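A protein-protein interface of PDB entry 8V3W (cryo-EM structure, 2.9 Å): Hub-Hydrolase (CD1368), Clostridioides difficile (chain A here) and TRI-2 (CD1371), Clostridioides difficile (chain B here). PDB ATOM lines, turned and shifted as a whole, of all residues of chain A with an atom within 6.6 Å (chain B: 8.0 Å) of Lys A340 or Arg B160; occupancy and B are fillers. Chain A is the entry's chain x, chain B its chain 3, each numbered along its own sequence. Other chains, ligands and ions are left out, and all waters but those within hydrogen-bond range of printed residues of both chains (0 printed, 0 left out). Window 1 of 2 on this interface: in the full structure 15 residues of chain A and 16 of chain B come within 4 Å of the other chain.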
ATOM      1  N   ALA A 337      -8.875  19.667 -26.691  1.00  0.00           N
ATOM      2  CA  ALA A 337      -7.489  19.611 -27.134  1.00  0.00           C
ATOM      3  C   ALA A 337      -6.583  19.540 -25.915  1.00  0.00           C
ATOM      4  O   ALA A 337      -6.995  19.835 -24.791  1.00  0.00           O
ATOM      5  CB  ALA A 337      -7.127  20.817 -28.009  1.00  0.00           C
ATOM      6  N   GLY A 338      -5.332  19.152 -26.157  1.00  0.00           N
ATOM      7  CA  GLY A 338      -4.390  18.934 -25.078  1.00  0.00           C
ATOM      8  C   GLY A 338      -4.520  17.595 -24.395  1.00  0.00           C
ATOM      9  O   GLY A 338      -3.928  17.397 -23.328  1.00  0.00           O
ATOM     10  N   GLY A 339      -5.264  16.666 -24.987  1.00  0.00           N
ATOM     11  CA  GLY A 339      -5.572  15.390 -24.376  1.00  0.00           C
ATOM     12  C   GLY A 339      -4.482  14.350 -24.514  1.00  0.00           C
ATOM     13  O   GLY A 339      -4.548  13.492 -25.399  1.00  0.00           O
ATOM     14  N   LYS A 340      -3.461  14.432 -23.664  1.00  0.00           N
ATOM     15  CA  LYS A 340      -2.397  13.440 -23.682  1.00  0.00           C
ATOM     16  C   LYS A 340      -2.973  12.040 -23.509  1.00  0.00           C
ATOM     17  O   LYS A 340      -3.884  11.816 -22.707  1.00  0.00           O
ATOM     18  CB  LYS A 340      -1.377  13.735 -22.583  1.00  0.00           C
ATOM     19  CG  LYS A 340      -0.427  14.878 -22.909  1.00  0.00           C
ATOM     20  CD  LYS A 340       0.862  14.354 -23.521  1.00  0.00           C
ATOM     21  CE  LYS A 340       1.461  13.230 -22.685  1.00  0.00           C
ATOM     22  NZ  LYS A 340       2.602  12.574 -23.378  1.00  0.00           N
ATOM     23  N   GLU A 341      -2.441  11.098 -24.280  1.00  0.00           N
ATOM     24  CA  GLU A 341      -2.979   9.747 -24.370  1.00  0.00           C
ATOM     25  C   GLU A 341      -2.091   8.787 -23.590  1.00  0.00           C
ATOM     26  O   GLU A 341      -0.879   8.732 -23.817  1.00  0.00           O
ATOM     27  CB  GLU A 341      -3.072   9.317 -25.836  1.00  0.00           C
ATOM     28  CG  GLU A 341      -4.216   8.377 -26.161  1.00  0.00           C
ATOM     29  CD  GLU A 341      -4.669   8.510 -27.602  1.00  0.00           C
ATOM     30  OE1 GLU A 341      -5.080   9.622 -27.992  1.00  0.00           O
ATOM     31  OE2 GLU A 341      -4.610   7.510 -28.346  1.00  0.00           O
ATOM     32  N   PHE A 342      -2.694   8.035 -22.674  1.00  0.00           N
ATOM     33  CA  PHE A 342      -1.974   7.068 -21.858  1.00  0.00           C
ATOM     34  C   PHE A 342      -2.604   5.692 -22.003  1.00  0.00           C
ATOM     35  O   PHE A 342      -3.831   5.560 -22.043  1.00  0.00           O
ATOM     36  CB  PHE A 342      -1.948   7.462 -20.366  1.00  0.00           C
ATOM     37  CG  PHE A 342      -1.603   8.908 -20.107  1.00  0.00           C
ATOM     38  CD1 PHE A 342      -2.494   9.926 -20.403  1.00  0.00           C
ATOM     39  CD2 PHE A 342      -0.381   9.242 -19.549  1.00  0.00           C
ATOM     40  CE1 PHE A 342      -2.166  11.245 -20.159  1.00  0.00           C
ATOM     41  CE2 PHE A 342      -0.050  10.559 -19.300  1.00  0.00           C
ATOM     42  CZ  PHE A 342      -0.946  11.561 -19.605  1.00  0.00           C
ATOM     43  N   THR A 343      -1.753   4.673 -22.090  1.00  0.00           N
ATOM     44  CA  THR A 343      -2.219   3.294 -22.081  1.00  0.00           C
ATOM     45  C   THR A 343      -2.773   2.943 -20.706  1.00  0.00           C
ATOM     46  O   THR A 343      -2.214   3.333 -19.677  1.00  0.00           O
ATOM     47  CB  THR A 343      -1.077   2.348 -22.452  1.00  0.00           C
ATOM     48  OG1 THR A 343      -0.471   2.790 -23.674  1.00  0.00           O
ATOM     49  CG2 THR A 343      -1.585   0.925 -22.629  1.00  0.00           C
ATOM     50  N   GLU A 389       9.916  13.567 -11.280  1.00  0.00           N
ATOM     51  CA  GLU A 389      10.022  13.392 -12.725  1.00  0.00           C
ATOM     52  C   GLU A 389       8.916  12.484 -13.244  1.00  0.00           C
ATOM     53  O   GLU A 389       8.263  12.787 -14.250  1.00  0.00           O
ATOM     54  CB  GLU A 389      11.393  12.818 -13.076  1.00  0.00           C
ATOM     55  CG  GLU A 389      11.504  12.310 -14.503  1.00  0.00           C
ATOM     56  CD  GLU A 389      12.762  11.502 -14.734  1.00  0.00           C
ATOM     57  OE1 GLU A 389      13.626  11.476 -13.833  1.00  0.00           O
ATOM     58  OE2 GLU A 389      12.886  10.888 -15.815  1.00  0.00           O
ATOM     59  N   PHE A 390       8.687  11.362 -12.559  1.00  0.00           N
ATOM     60  CA  PHE A 390       7.642  10.432 -12.974  1.00  0.00           C
ATOM     61  C   PHE A 390       6.262  11.063 -12.853  1.00  0.00           C
ATOM     62  O   PHE A 390       5.416  10.895 -13.740  1.00  0.00           O
ATOM     63  CB  PHE A 390       7.732   9.155 -12.138  1.00  0.00           C
ATOM     64  CG  PHE A 390       6.877   8.032 -12.643  1.00  0.00           C
ATOM     65  CD1 PHE A 390       7.317   7.222 -13.677  1.00  0.00           C
ATOM     66  CD2 PHE A 390       5.647   7.767 -12.065  1.00  0.00           C
ATOM     67  CE1 PHE A 390       6.538   6.177 -14.139  1.00  0.00           C
ATOM     68  CE2 PHE A 390       4.863   6.724 -12.522  1.00  0.00           C
ATOM     69  CZ  PHE A 390       5.309   5.927 -13.560  1.00  0.00           C
ATOM     70  N   ASN A 392       5.474  14.281 -12.975  1.00  0.00           N
ATOM     71  CA  ASN A 392       5.321  15.242 -14.061  1.00  0.00           C
ATOM     72  C   ASN A 392       5.130  14.538 -15.397  1.00  0.00           C
ATOM     73  O   ASN A 392       4.439  15.060 -16.280  1.00  0.00           O
ATOM     74  CB  ASN A 392       6.532  16.173 -14.119  1.00  0.00           C
ATOM     75  CG  ASN A 392       6.500  17.236 -13.040  1.00  0.00           C
ATOM     76  OD1 ASN A 392       5.495  17.406 -12.350  1.00  0.00           O
ATOM     77  ND2 ASN A 392       7.603  17.962 -12.891  1.00  0.00           N
ATOM     78  N   LYS A 393       5.731  13.361 -15.562  1.00  0.00           N
ATOM     79  CA  LYS A 393       5.573  12.607 -16.799  1.00  0.00           C
ATOM     80  C   LYS A 393       4.255  11.841 -16.824  1.00  0.00           C
ATOM     81  O   LYS A 393       3.615  11.735 -17.876  1.00  0.00           O
ATOM     82  CB  LYS A 393       6.758  11.658 -16.980  1.00  0.00           C
ATOM     83  CG  LYS A 393       8.017  12.362 -17.461  1.00  0.00           C
ATOM     84  CD  LYS A 393       8.983  11.407 -18.137  1.00  0.00           C
ATOM     85  CE  LYS A 393      10.084  12.172 -18.856  1.00  0.00           C
ATOM     86  NZ  LYS A 393      10.913  11.285 -19.712  1.00  0.00           N
ATOM     87  N   HIS A 394       3.832  11.305 -15.678  1.00  0.00           N
ATOM     88  CA  HIS A 394       2.554  10.610 -15.535  1.00  0.00           C
ATOM     89  C   HIS A 394       1.767  11.309 -14.435  1.00  0.00           C
ATOM     90  O   HIS A 394       1.903  10.968 -13.249  1.00  0.00           O
ATOM     91  CB  HIS A 394       2.758   9.131 -15.214  1.00  0.00           C
ATOM     92  CG  HIS A 394       3.450   8.364 -16.297  1.00  0.00           C
ATOM     93  ND1 HIS A 394       4.745   7.913 -16.178  1.00  0.00           N
ATOM     94  CD2 HIS A 394       3.022   7.962 -17.517  1.00  0.00           C
ATOM     95  CE1 HIS A 394       5.089   7.269 -17.279  1.00  0.00           C
ATOM     96  NE2 HIS A 394       4.061   7.284 -18.107  1.00  0.00           N
ATOM     97  N   GLN A 404     -11.579  10.518 -20.721  1.00  0.00           N
ATOM     98  CA  GLN A 404     -12.174   9.758 -21.812  1.00  0.00           C
ATOM     99  C   GLN A 404     -11.584   8.354 -21.839  1.00  0.00           C
ATOM    100  O   GLN A 404     -10.362   8.187 -21.930  1.00  0.00           O
ATOM    101  CB  GLN A 404     -11.966  10.479 -23.145  1.00  0.00           C
ATOM    102  CG  GLN A 404     -12.311  11.969 -23.093  1.00  0.00           C
ATOM    103  CD  GLN A 404     -11.107  12.856 -22.867  1.00  0.00           C
ATOM    104  OE1 GLN A 404     -10.015  12.374 -22.594  1.00  0.00           O
ATOM    105  NE2 GLN A 404     -11.302  14.164 -22.983  1.00  0.00           N
ATOM    106  N   ASN A 430       5.958   1.195 -16.029  1.00  0.00           N
ATOM    107  CA  ASN A 430       5.981   1.553 -17.443  1.00  0.00           C
ATOM    108  C   ASN A 430       5.039   2.707 -17.758  1.00  0.00           C
ATOM    109  O   ASN A 430       5.177   3.333 -18.814  1.00  0.00           O
ATOM    110  CB  ASN A 430       5.636   0.337 -18.309  1.00  0.00           C
ATOM    111  CG  ASN A 430       4.229  -0.186 -18.066  1.00  0.00           C
ATOM    112  OD1 ASN A 430       3.473   0.357 -17.259  1.00  0.00           O
ATOM    113  ND2 ASN A 430       3.876  -1.258 -18.762  1.00  0.00           N
ATOM    114  N   GLY A 431       4.094   3.002 -16.871  1.00  0.00           N
ATOM    115  CA  GLY A 431       3.147   4.076 -17.075  1.00  0.00           C
ATOM    116  C   GLY A 431       1.726   3.652 -17.376  1.00  0.00           C
ATOM    117  O   GLY A 431       0.900   4.514 -17.692  1.00  0.00           O
ATOM    118  N   ILE A 455      -6.675   5.506 -22.122  1.00  0.00           N
ATOM    119  CA  ILE A 455      -7.454   6.611 -21.586  1.00  0.00           C
ATOM    120  C   ILE A 455      -6.732   7.911 -21.908  1.00  0.00           C
ATOM    121  O   ILE A 455      -5.529   7.935 -22.175  1.00  0.00           O
ATOM    122  CB  ILE A 455      -7.685   6.507 -20.066  1.00  0.00           C
ATOM    123  CG1 ILE A 455      -6.351   6.406 -19.331  1.00  0.00           C
ATOM    124  CG2 ILE A 455      -8.563   5.314 -19.741  1.00  0.00           C
ATOM    125  CD1 ILE A 455      -6.440   6.804 -17.885  1.00  0.00           C
ATOM    126  N   ILE A 456      -7.492   8.999 -21.875  1.00  0.00           N
ATOM    127  CA  ILE A 456      -6.981  10.330 -22.167  1.00  0.00           C
ATOM    128  C   ILE A 456      -7.404  11.250 -21.030  1.00  0.00           C
ATOM    129  O   ILE A 456      -8.558  11.206 -20.590  1.00  0.00           O
ATOM    130  CB  ILE A 456      -7.501  10.846 -23.520  1.00  0.00           C
ATOM    131  CG1 ILE A 456      -6.981   9.969 -24.656  1.00  0.00           C
ATOM    132  CG2 ILE A 456      -7.074  12.276 -23.741  1.00  0.00           C
ATOM    133  CD1 ILE A 456      -7.643  10.242 -25.983  1.00  0.00           C
ATOM    134  N   ILE A 457      -6.465  12.056 -20.530  1.00  0.00           N
ATOM    135  CA  ILE A 457      -6.727  12.952 -19.414  1.00  0.00           C
ATOM    136  C   ILE A 457      -6.196  14.341 -19.739  1.00  0.00           C
ATOM    137  O   ILE A 457      -5.303  14.516 -20.572  1.00  0.00           O
ATOM    138  CB  ILE A 457      -6.107  12.445 -18.091  1.00  0.00           C
ATOM    139  CG1 ILE A 457      -4.581  12.546 -18.133  1.00  0.00           C
ATOM    140  CG2 ILE A 457      -6.546  11.019 -17.796  1.00  0.00           C
ATOM    141  CD1 ILE A 457      -4.003  13.620 -17.234  1.00  0.00           C
ATOM    142  N   GLY A 458      -6.765  15.334 -19.061  1.00  0.00           N
ATOM    143  CA  GLY A 458      -6.265  16.696 -19.144  1.00  0.00           C
ATOM    144  C   GLY A 458      -6.358  17.330 -20.513  1.00  0.00           C
ATOM    145  O   GLY A 458      -5.466  18.094 -20.894  1.00  0.00           O
ATOM    146  N   GLY A 459      -7.414  17.036 -21.267  1.00  0.00           N
ATOM    147  CA  GLY A 459      -7.612  17.679 -22.551  1.00  0.00           C
ATOM    148  C   GLY A 459      -8.875  18.511 -22.602  1.00  0.00           C
ATOM    149  O   GLY A 459      -9.982  17.963 -22.621  1.00  0.00           O
ATOM    150  N   ASN B  83       9.278  14.871 -29.799  1.00  0.00           N
ATOM    151  CA  ASN B  83       9.944  14.225 -28.679  1.00  0.00           C
ATOM    152  C   ASN B  83       9.002  13.208 -28.052  1.00  0.00           C
ATOM    153  O   ASN B  83       7.797  13.451 -27.938  1.00  0.00           O
ATOM    154  CB  ASN B  83      10.389  15.251 -27.633  1.00  0.00           C
ATOM    155  CG  ASN B  83      11.512  16.137 -28.131  1.00  0.00           C
ATOM    156  OD1 ASN B  83      12.672  15.725 -28.175  1.00  0.00           O
ATOM    157  ND2 ASN B  83      11.174  17.361 -28.517  1.00  0.00           N
ATOM    158  N   GLY B  84       9.555  12.065 -27.658  1.00  0.00           N
ATOM    159  CA  GLY B  84       8.746  11.012 -27.080  1.00  0.00           C
ATOM    160  C   GLY B  84       9.605  10.034 -26.310  1.00  0.00           C
ATOM    161  O   GLY B  84      10.833  10.143 -26.272  1.00  0.00           O
ATOM    162  N   GLU B  85       8.934   9.069 -25.685  1.00  0.00           N
ATOM    163  CA  GLU B  85       9.591   8.049 -24.880  1.00  0.00           C
ATOM    164  C   GLU B  85       8.989   6.693 -25.215  1.00  0.00           C
ATOM    165  O   GLU B  85       7.766   6.563 -25.314  1.00  0.00           O
ATOM    166  CB  GLU B  85       9.432   8.343 -23.384  1.00  0.00           C
ATOM    167  CG  GLU B  85      10.294   7.484 -22.475  1.00  0.00           C
ATOM    168  CD  GLU B  85      10.022   7.749 -21.007  1.00  0.00           C
ATOM    169  OE1 GLU B  85       9.136   7.079 -20.436  1.00  0.00           O
ATOM    170  OE2 GLU B  85      10.683   8.634 -20.427  1.00  0.00           O
ATOM    171  N   VAL B  86       9.847   5.689 -25.387  1.00  0.00           N
ATOM    172  CA  VAL B  86       9.416   4.329 -25.674  1.00  0.00           C
ATOM    173  C   VAL B  86       9.995   3.398 -24.614  1.00  0.00           C
ATOM    174  O   VAL B  86      10.892   3.761 -23.853  1.00  0.00           O
ATOM    175  CB  VAL B  86       9.825   3.865 -27.083  1.00  0.00           C
ATOM    176  CG1 VAL B  86       9.370   4.868 -28.130  1.00  0.00           C
ATOM    177  CG2 VAL B  86      11.326   3.646 -27.153  1.00  0.00           C
ATOM    178  N   ASN B 124      12.802   2.742 -20.050  1.00  0.00           N
ATOM    179  CA  ASN B 124      12.280   3.839 -20.852  1.00  0.00           C
ATOM    180  C   ASN B 124      13.378   4.862 -21.105  1.00  0.00           C
ATOM    181  O   ASN B 124      14.040   5.316 -20.166  1.00  0.00           O
ATOM    182  CB  ASN B 124      11.088   4.500 -20.159  1.00  0.00           C
ATOM    183  CG  ASN B 124       9.837   3.650 -20.223  1.00  0.00           C
ATOM    184  OD1 ASN B 124       9.300   3.399 -21.301  1.00  0.00           O
ATOM    185  ND2 ASN B 124       9.366   3.199 -19.066  1.00  0.00           N
ATOM    186  N   ASN B 137       4.178  12.889 -34.852  1.00  0.00           N
ATOM    187  CA  ASN B 137       3.460  12.857 -33.578  1.00  0.00           C
ATOM    188  C   ASN B 137       2.609  11.589 -33.518  1.00  0.00           C
ATOM    189  O   ASN B 137       1.385  11.600 -33.663  1.00  0.00           O
ATOM    190  CB  ASN B 137       2.617  14.111 -33.407  1.00  0.00           C
ATOM    191  CG  ASN B 137       3.448  15.333 -33.084  1.00  0.00           C
ATOM    192  OD1 ASN B 137       4.641  15.231 -32.805  1.00  0.00           O
ATOM    193  ND2 ASN B 137       2.820  16.501 -33.124  1.00  0.00           N
ATOM    194  N   LEU B 138       3.295  10.473 -33.296  1.00  0.00           N
ATOM    195  CA  LEU B 138       2.649   9.174 -33.301  1.00  0.00           C
ATOM    196  C   LEU B 138       1.728   9.012 -32.093  1.00  0.00           C
ATOM    197  O   LEU B 138       2.009   9.532 -31.010  1.00  0.00           O
ATOM    198  CB  LEU B 138       3.696   8.067 -33.294  1.00  0.00           C
ATOM    199  CG  LEU B 138       4.147   7.509 -34.640  1.00  0.00           C
ATOM    200  CD1 LEU B 138       4.949   8.534 -35.416  1.00  0.00           C
ATOM    201  CD2 LEU B 138       4.983   6.277 -34.383  1.00  0.00           C
ATOM    202  N   PRO B 139       0.621   8.284 -32.255  1.00  0.00           N
ATOM    203  CA  PRO B 139      -0.239   7.982 -31.104  1.00  0.00           C
ATOM    204  C   PRO B 139       0.386   6.938 -30.195  1.00  0.00           C
ATOM    205  O   PRO B 139       1.521   6.508 -30.426  1.00  0.00           O
ATOM    206  CB  PRO B 139      -1.524   7.462 -31.757  1.00  0.00           C
ATOM    207  CG  PRO B 139      -1.074   6.915 -33.071  1.00  0.00           C
ATOM    208  CD  PRO B 139       0.050   7.797 -33.521  1.00  0.00           C
ATOM    209  N   THR B 140      -0.333   6.522 -29.157  1.00  0.00           N
ATOM    210  CA  THR B 140       0.235   5.560 -28.229  1.00  0.00           C
ATOM    211  C   THR B 140       0.087   4.139 -28.769  1.00  0.00           C
ATOM    212  O   THR B 140      -0.562   3.892 -29.788  1.00  0.00           O
ATOM    213  CB  THR B 140      -0.416   5.670 -26.854  1.00  0.00           C
ATOM    214  OG1 THR B 140       0.277   4.820 -25.934  1.00  0.00           O
ATOM    215  CG2 THR B 140      -1.863   5.230 -26.921  1.00  0.00           C
ATOM    216  N   ASN B 141       0.716   3.200 -28.061  1.00  0.00           N
ATOM    217  CA  ASN B 141       0.641   1.774 -28.380  1.00  0.00           C
ATOM    218  C   ASN B 141       1.114   1.491 -29.804  1.00  0.00           C
ATOM    219  O   ASN B 141       0.576   0.624 -30.496  1.00  0.00           O
ATOM    220  CB  ASN B 141      -0.773   1.233 -28.161  1.00  0.00           C
ATOM    221  CG  ASN B 141      -1.135   1.132 -26.694  1.00  0.00           C
ATOM    222  OD1 ASN B 141      -0.322   1.429 -25.819  1.00  0.00           O
ATOM    223  ND2 ASN B 141      -2.361   0.709 -26.416  1.00  0.00           N
ATOM    224  N   CYS B 142       2.128   2.226 -30.245  1.00  0.00           N
ATOM    225  CA  CYS B 142       2.740   2.003 -31.548  1.00  0.00           C
ATOM    226  C   CYS B 142       3.968   1.122 -31.372  1.00  0.00           C
ATOM    227  O   CYS B 142       4.849   1.433 -30.565  1.00  0.00           O
ATOM    228  CB  CYS B 142       3.123   3.327 -32.211  1.00  0.00           C
ATOM    229  SG  CYS B 142       1.725   4.296 -32.813  1.00  0.00           S
ATOM    230  N   PHE B 144       7.328   0.021 -32.309  1.00  0.00           N
ATOM    231  CA  PHE B 144       8.506   0.454 -33.041  1.00  0.00           C
ATOM    232  C   PHE B 144       9.412  -0.735 -33.340  1.00  0.00           C
ATOM    233  O   PHE B 144       9.428  -1.734 -32.619  1.00  0.00           O
ATOM    234  CB  PHE B 144       9.282   1.510 -32.253  1.00  0.00           C
ATOM    235  CG  PHE B 144       8.521   2.782 -32.022  1.00  0.00           C
ATOM    236  CD1 PHE B 144       7.595   2.878 -30.998  1.00  0.00           C
ATOM    237  CD2 PHE B 144       8.747   3.890 -32.817  1.00  0.00           C
ATOM    238  CE1 PHE B 144       6.901   4.049 -30.782  1.00  0.00           C
ATOM    239  CE2 PHE B 144       8.060   5.065 -32.605  1.00  0.00           C
ATOM    240  CZ  PHE B 144       7.135   5.145 -31.586  1.00  0.00           C
ATOM    241  N   THR B 157       7.675  -0.215 -27.765  1.00  0.00           N
ATOM    242  CA  THR B 157       6.374   0.438 -27.789  1.00  0.00           C
ATOM    243  C   THR B 157       6.453   1.738 -27.008  1.00  0.00           C
ATOM    244  O   THR B 157       7.314   1.918 -26.143  1.00  0.00           O
ATOM    245  CB  THR B 157       5.274  -0.458 -27.208  1.00  0.00           C
ATOM    246  OG1 THR B 157       4.063   0.297 -27.080  1.00  0.00           O
ATOM    247  CG2 THR B 157       5.684  -0.988 -25.846  1.00  0.00           C
ATOM    248  N   ASN B 158       5.534   2.645 -27.321  1.00  0.00           N
ATOM    249  CA  ASN B 158       5.422   3.923 -26.637  1.00  0.00           C
ATOM    250  C   ASN B 158       4.231   3.888 -25.687  1.00  0.00           C
ATOM    251  O   ASN B 158       3.194   3.292 -25.996  1.00  0.00           O
ATOM    252  CB  ASN B 158       5.270   5.073 -27.637  1.00  0.00           C
ATOM    253  CG  ASN B 158       3.916   5.086 -28.312  1.00  0.00           C
ATOM    254  OD1 ASN B 158       3.397   4.044 -28.712  1.00  0.00           O
ATOM    255  ND2 ASN B 158       3.337   6.272 -28.447  1.00  0.00           N
ATOM    256  N   THR B 159       4.393   4.514 -24.525  1.00  0.00           N
ATOM    257  CA  THR B 159       3.347   4.517 -23.514  1.00  0.00           C
ATOM    258  C   THR B 159       2.460   5.751 -23.579  1.00  0.00           C
ATOM    259  O   THR B 159       1.322   5.705 -23.097  1.00  0.00           O
ATOM    260  CB  THR B 159       3.966   4.412 -22.119  1.00  0.00           C
ATOM    261  OG1 THR B 159       4.816   5.542 -21.887  1.00  0.00           O
ATOM    262  CG2 THR B 159       4.791   3.139 -22.009  1.00  0.00           C
ATOM    263  N   ARG B 160       2.947   6.844 -24.162  1.00  0.00           N
ATOM    264  CA  ARG B 160       2.167   8.060 -24.340  1.00  0.00           C
ATOM    265  C   ARG B 160       2.224   8.474 -25.804  1.00  0.00           C
ATOM    266  O   ARG B 160       2.821   7.795 -26.645  1.00  0.00           O
ATOM    267  CB  ARG B 160       2.674   9.194 -23.439  1.00  0.00           C
ATOM    268  CG  ARG B 160       2.984   8.777 -22.016  1.00  0.00           C
ATOM    269  CD  ARG B 160       3.795   9.844 -21.309  1.00  0.00           C
ATOM    270  NE  ARG B 160       4.842   9.265 -20.476  1.00  0.00           N
ATOM    271  CZ  ARG B 160       5.856   9.950 -19.966  1.00  0.00           C
ATOM    272  NH1 ARG B 160       5.981  11.252 -20.166  1.00  0.00           N
ATOM    273  NH2 ARG B 160       6.770   9.311 -19.242  1.00  0.00           N
ATOM    274  N   SER B 161       1.595   9.603 -26.107  1.00  0.00           N
ATOM    275  CA  SER B 161       1.584  10.142 -27.456  1.00  0.00           C
ATOM    276  C   SER B 161       2.811  11.012 -27.691  1.00  0.00           C
ATOM    277  O   SER B 161       3.353  11.624 -26.766  1.00  0.00           O
ATOM    278  CB  SER B 161       0.315  10.957 -27.703  1.00  0.00           C
ATOM    279  OG  SER B 161       0.272  12.095 -26.861  1.00  0.00           O
ATOM    280  N   PHE B 162       3.249  11.059 -28.945  1.00  0.00           N
ATOM    281  CA  PHE B 162       4.379  11.896 -29.318  1.00  0.00           C
ATOM    282  C   PHE B 162       3.925  13.335 -29.509  1.00  0.00           C
ATOM    283  O   PHE B 162       2.839  13.595 -30.035  1.00  0.00           O
ATOM    284  CB  PHE B 162       5.034  11.376 -30.596  1.00  0.00           C
ATOM    285  CG  PHE B 162       5.936  10.197 -30.377  1.00  0.00           C
ATOM    286  CD1 PHE B 162       5.439   9.010 -29.866  1.00  0.00           C
ATOM    287  CD2 PHE B 162       7.283  10.279 -30.678  1.00  0.00           C
ATOM    288  CE1 PHE B 162       6.268   7.928 -29.665  1.00  0.00           C
ATOM    289  CE2 PHE B 162       8.116   9.200 -30.479  1.00  0.00           C
ATOM    290  CZ  PHE B 162       7.610   8.023 -29.970  1.00  0.00           C
ATOM    291  N   GLU B 163       4.763  14.273 -29.077  1.00  0.00           N
ATOM    292  CA  GLU B 163       4.438  15.689 -29.144  1.00  0.00           C
ATOM    293  C   GLU B 163       5.698  16.485 -29.448  1.00  0.00           C
ATOM    294  O   GLU B 163       6.820  16.013 -29.247  1.00  0.00           O
ATOM    295  CB  GLU B 163       3.804  16.185 -27.837  1.00  0.00           C
ATOM    296  CG  GLU B 163       4.599  15.819 -26.596  1.00  0.00           C
ATOM    297  CD  GLU B 163       4.185  16.618 -25.375  1.00  0.00           C
ATOM    298  OE1 GLU B 163       3.424  17.594 -25.529  1.00  0.00           O
ATOM    299  OE2 GLU B 163       4.627  16.271 -24.261  1.00  0.00           O
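NZ of Lys A393 is in salt-bridge range of OE2 of Glu B85 (2.8 Å). The side-chain hydroxyl (OG1) of Thr A343 is in hydrogen-bond range of the side-chain hydroxyl (OG1) of Thr B140. OD1 of Asn B141 sits at hydrogen-bond distance from OG1 of Thr A343, 2.5 Å away. N of Thr A343 sits at hydrogen-bond distance from O of Thr B159 (3.4 Å). The backbone carbonyl oxygen of Lys A393 lies close to the guanidinium group of Arg B160 (3.3 Å). The guanidinium group (NE) of Arg B160 sits at hydrogen-bond distance from a ring nitrogen (NE2) of His A394, at 3.2 Å. The backbone NH (N) of Ser B161 lies within hydrogen-bond range of the backbone carbonyl oxygen (O) of Glu A341.
The side-chain carboxylate (OE1) of Glu B85 lies within salt-bridge range of the guanidinium group (NH2) of Arg B160, at 3.5 Å. OG1 of Thr B140 lies within hydrogen-bond range of OD1 of Asn B141 (3.4 Å). OG1 of Thr B140 sits at hydrogen-bond distance from O of Asn B158 (3.3 Å). The side-chain hydroxyl (OG1) of Thr B140 sits at hydrogen-bond distance from the backbone carbonyl oxygen (O) of Thr B159 (3.2 Å). The backbone NH of Asn B141 sits at hydrogen-bond distance from the side-chain amide oxygen of Asn B158. N of Ile A457 lies within hydrogen-bond range of O of Lys A340 (3.4 Å).
Lys A340 touches Arg B160. NZ of Lys A340 touches O of Ser B161 (3.6 Å). Thr B140 touches Glu A341. Thr B159 touches Glu A341. Arg B160 touches Glu A341 (CA to O, 3.2 Å). O of Thr B159 touches CA of Phe A342 (3.8 Å). CG2 of Thr B159 touches O of Asn A430, at 3.2 Å.
Lys A340 touches just these residues of chain B: Arg B160 (3.4 Å) and Ser B161 (3.6 Å). No residue of chain B comes within 4 Å of Gly A339. Printed residues of chain A within 4 Å of Thr B159: Glu A341, Phe A342, Thr A343 and Asn A430. Printed residues of chain A within 4 Å of Ser B161: Lys A340 (3.6 Å) and Glu A341 (3.5 Å). Printed residues of chain B within 4 Å of Asn A430: Thr B159 (3.2 Å). The nearest residue of chain A that does not touch Arg B160 is Phe A342 (4.2 Å). The nearest printed residue of chain B that does not touch His A394 is Thr B159 (4.2 Å).
Hydrophobic or aromatic side chains of chain A that line the printed part of chain B: His A394. Of the 19 printed residues of chain B, 6 touch a printed residue of chain A. Printed residues of chain B that touch a printed residue of chain A: Glu B85, Thr B140, Asn B141, Thr B159, Arg B160 and Ser B161. Among the printed residues, 14 pairs touch across the chains.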
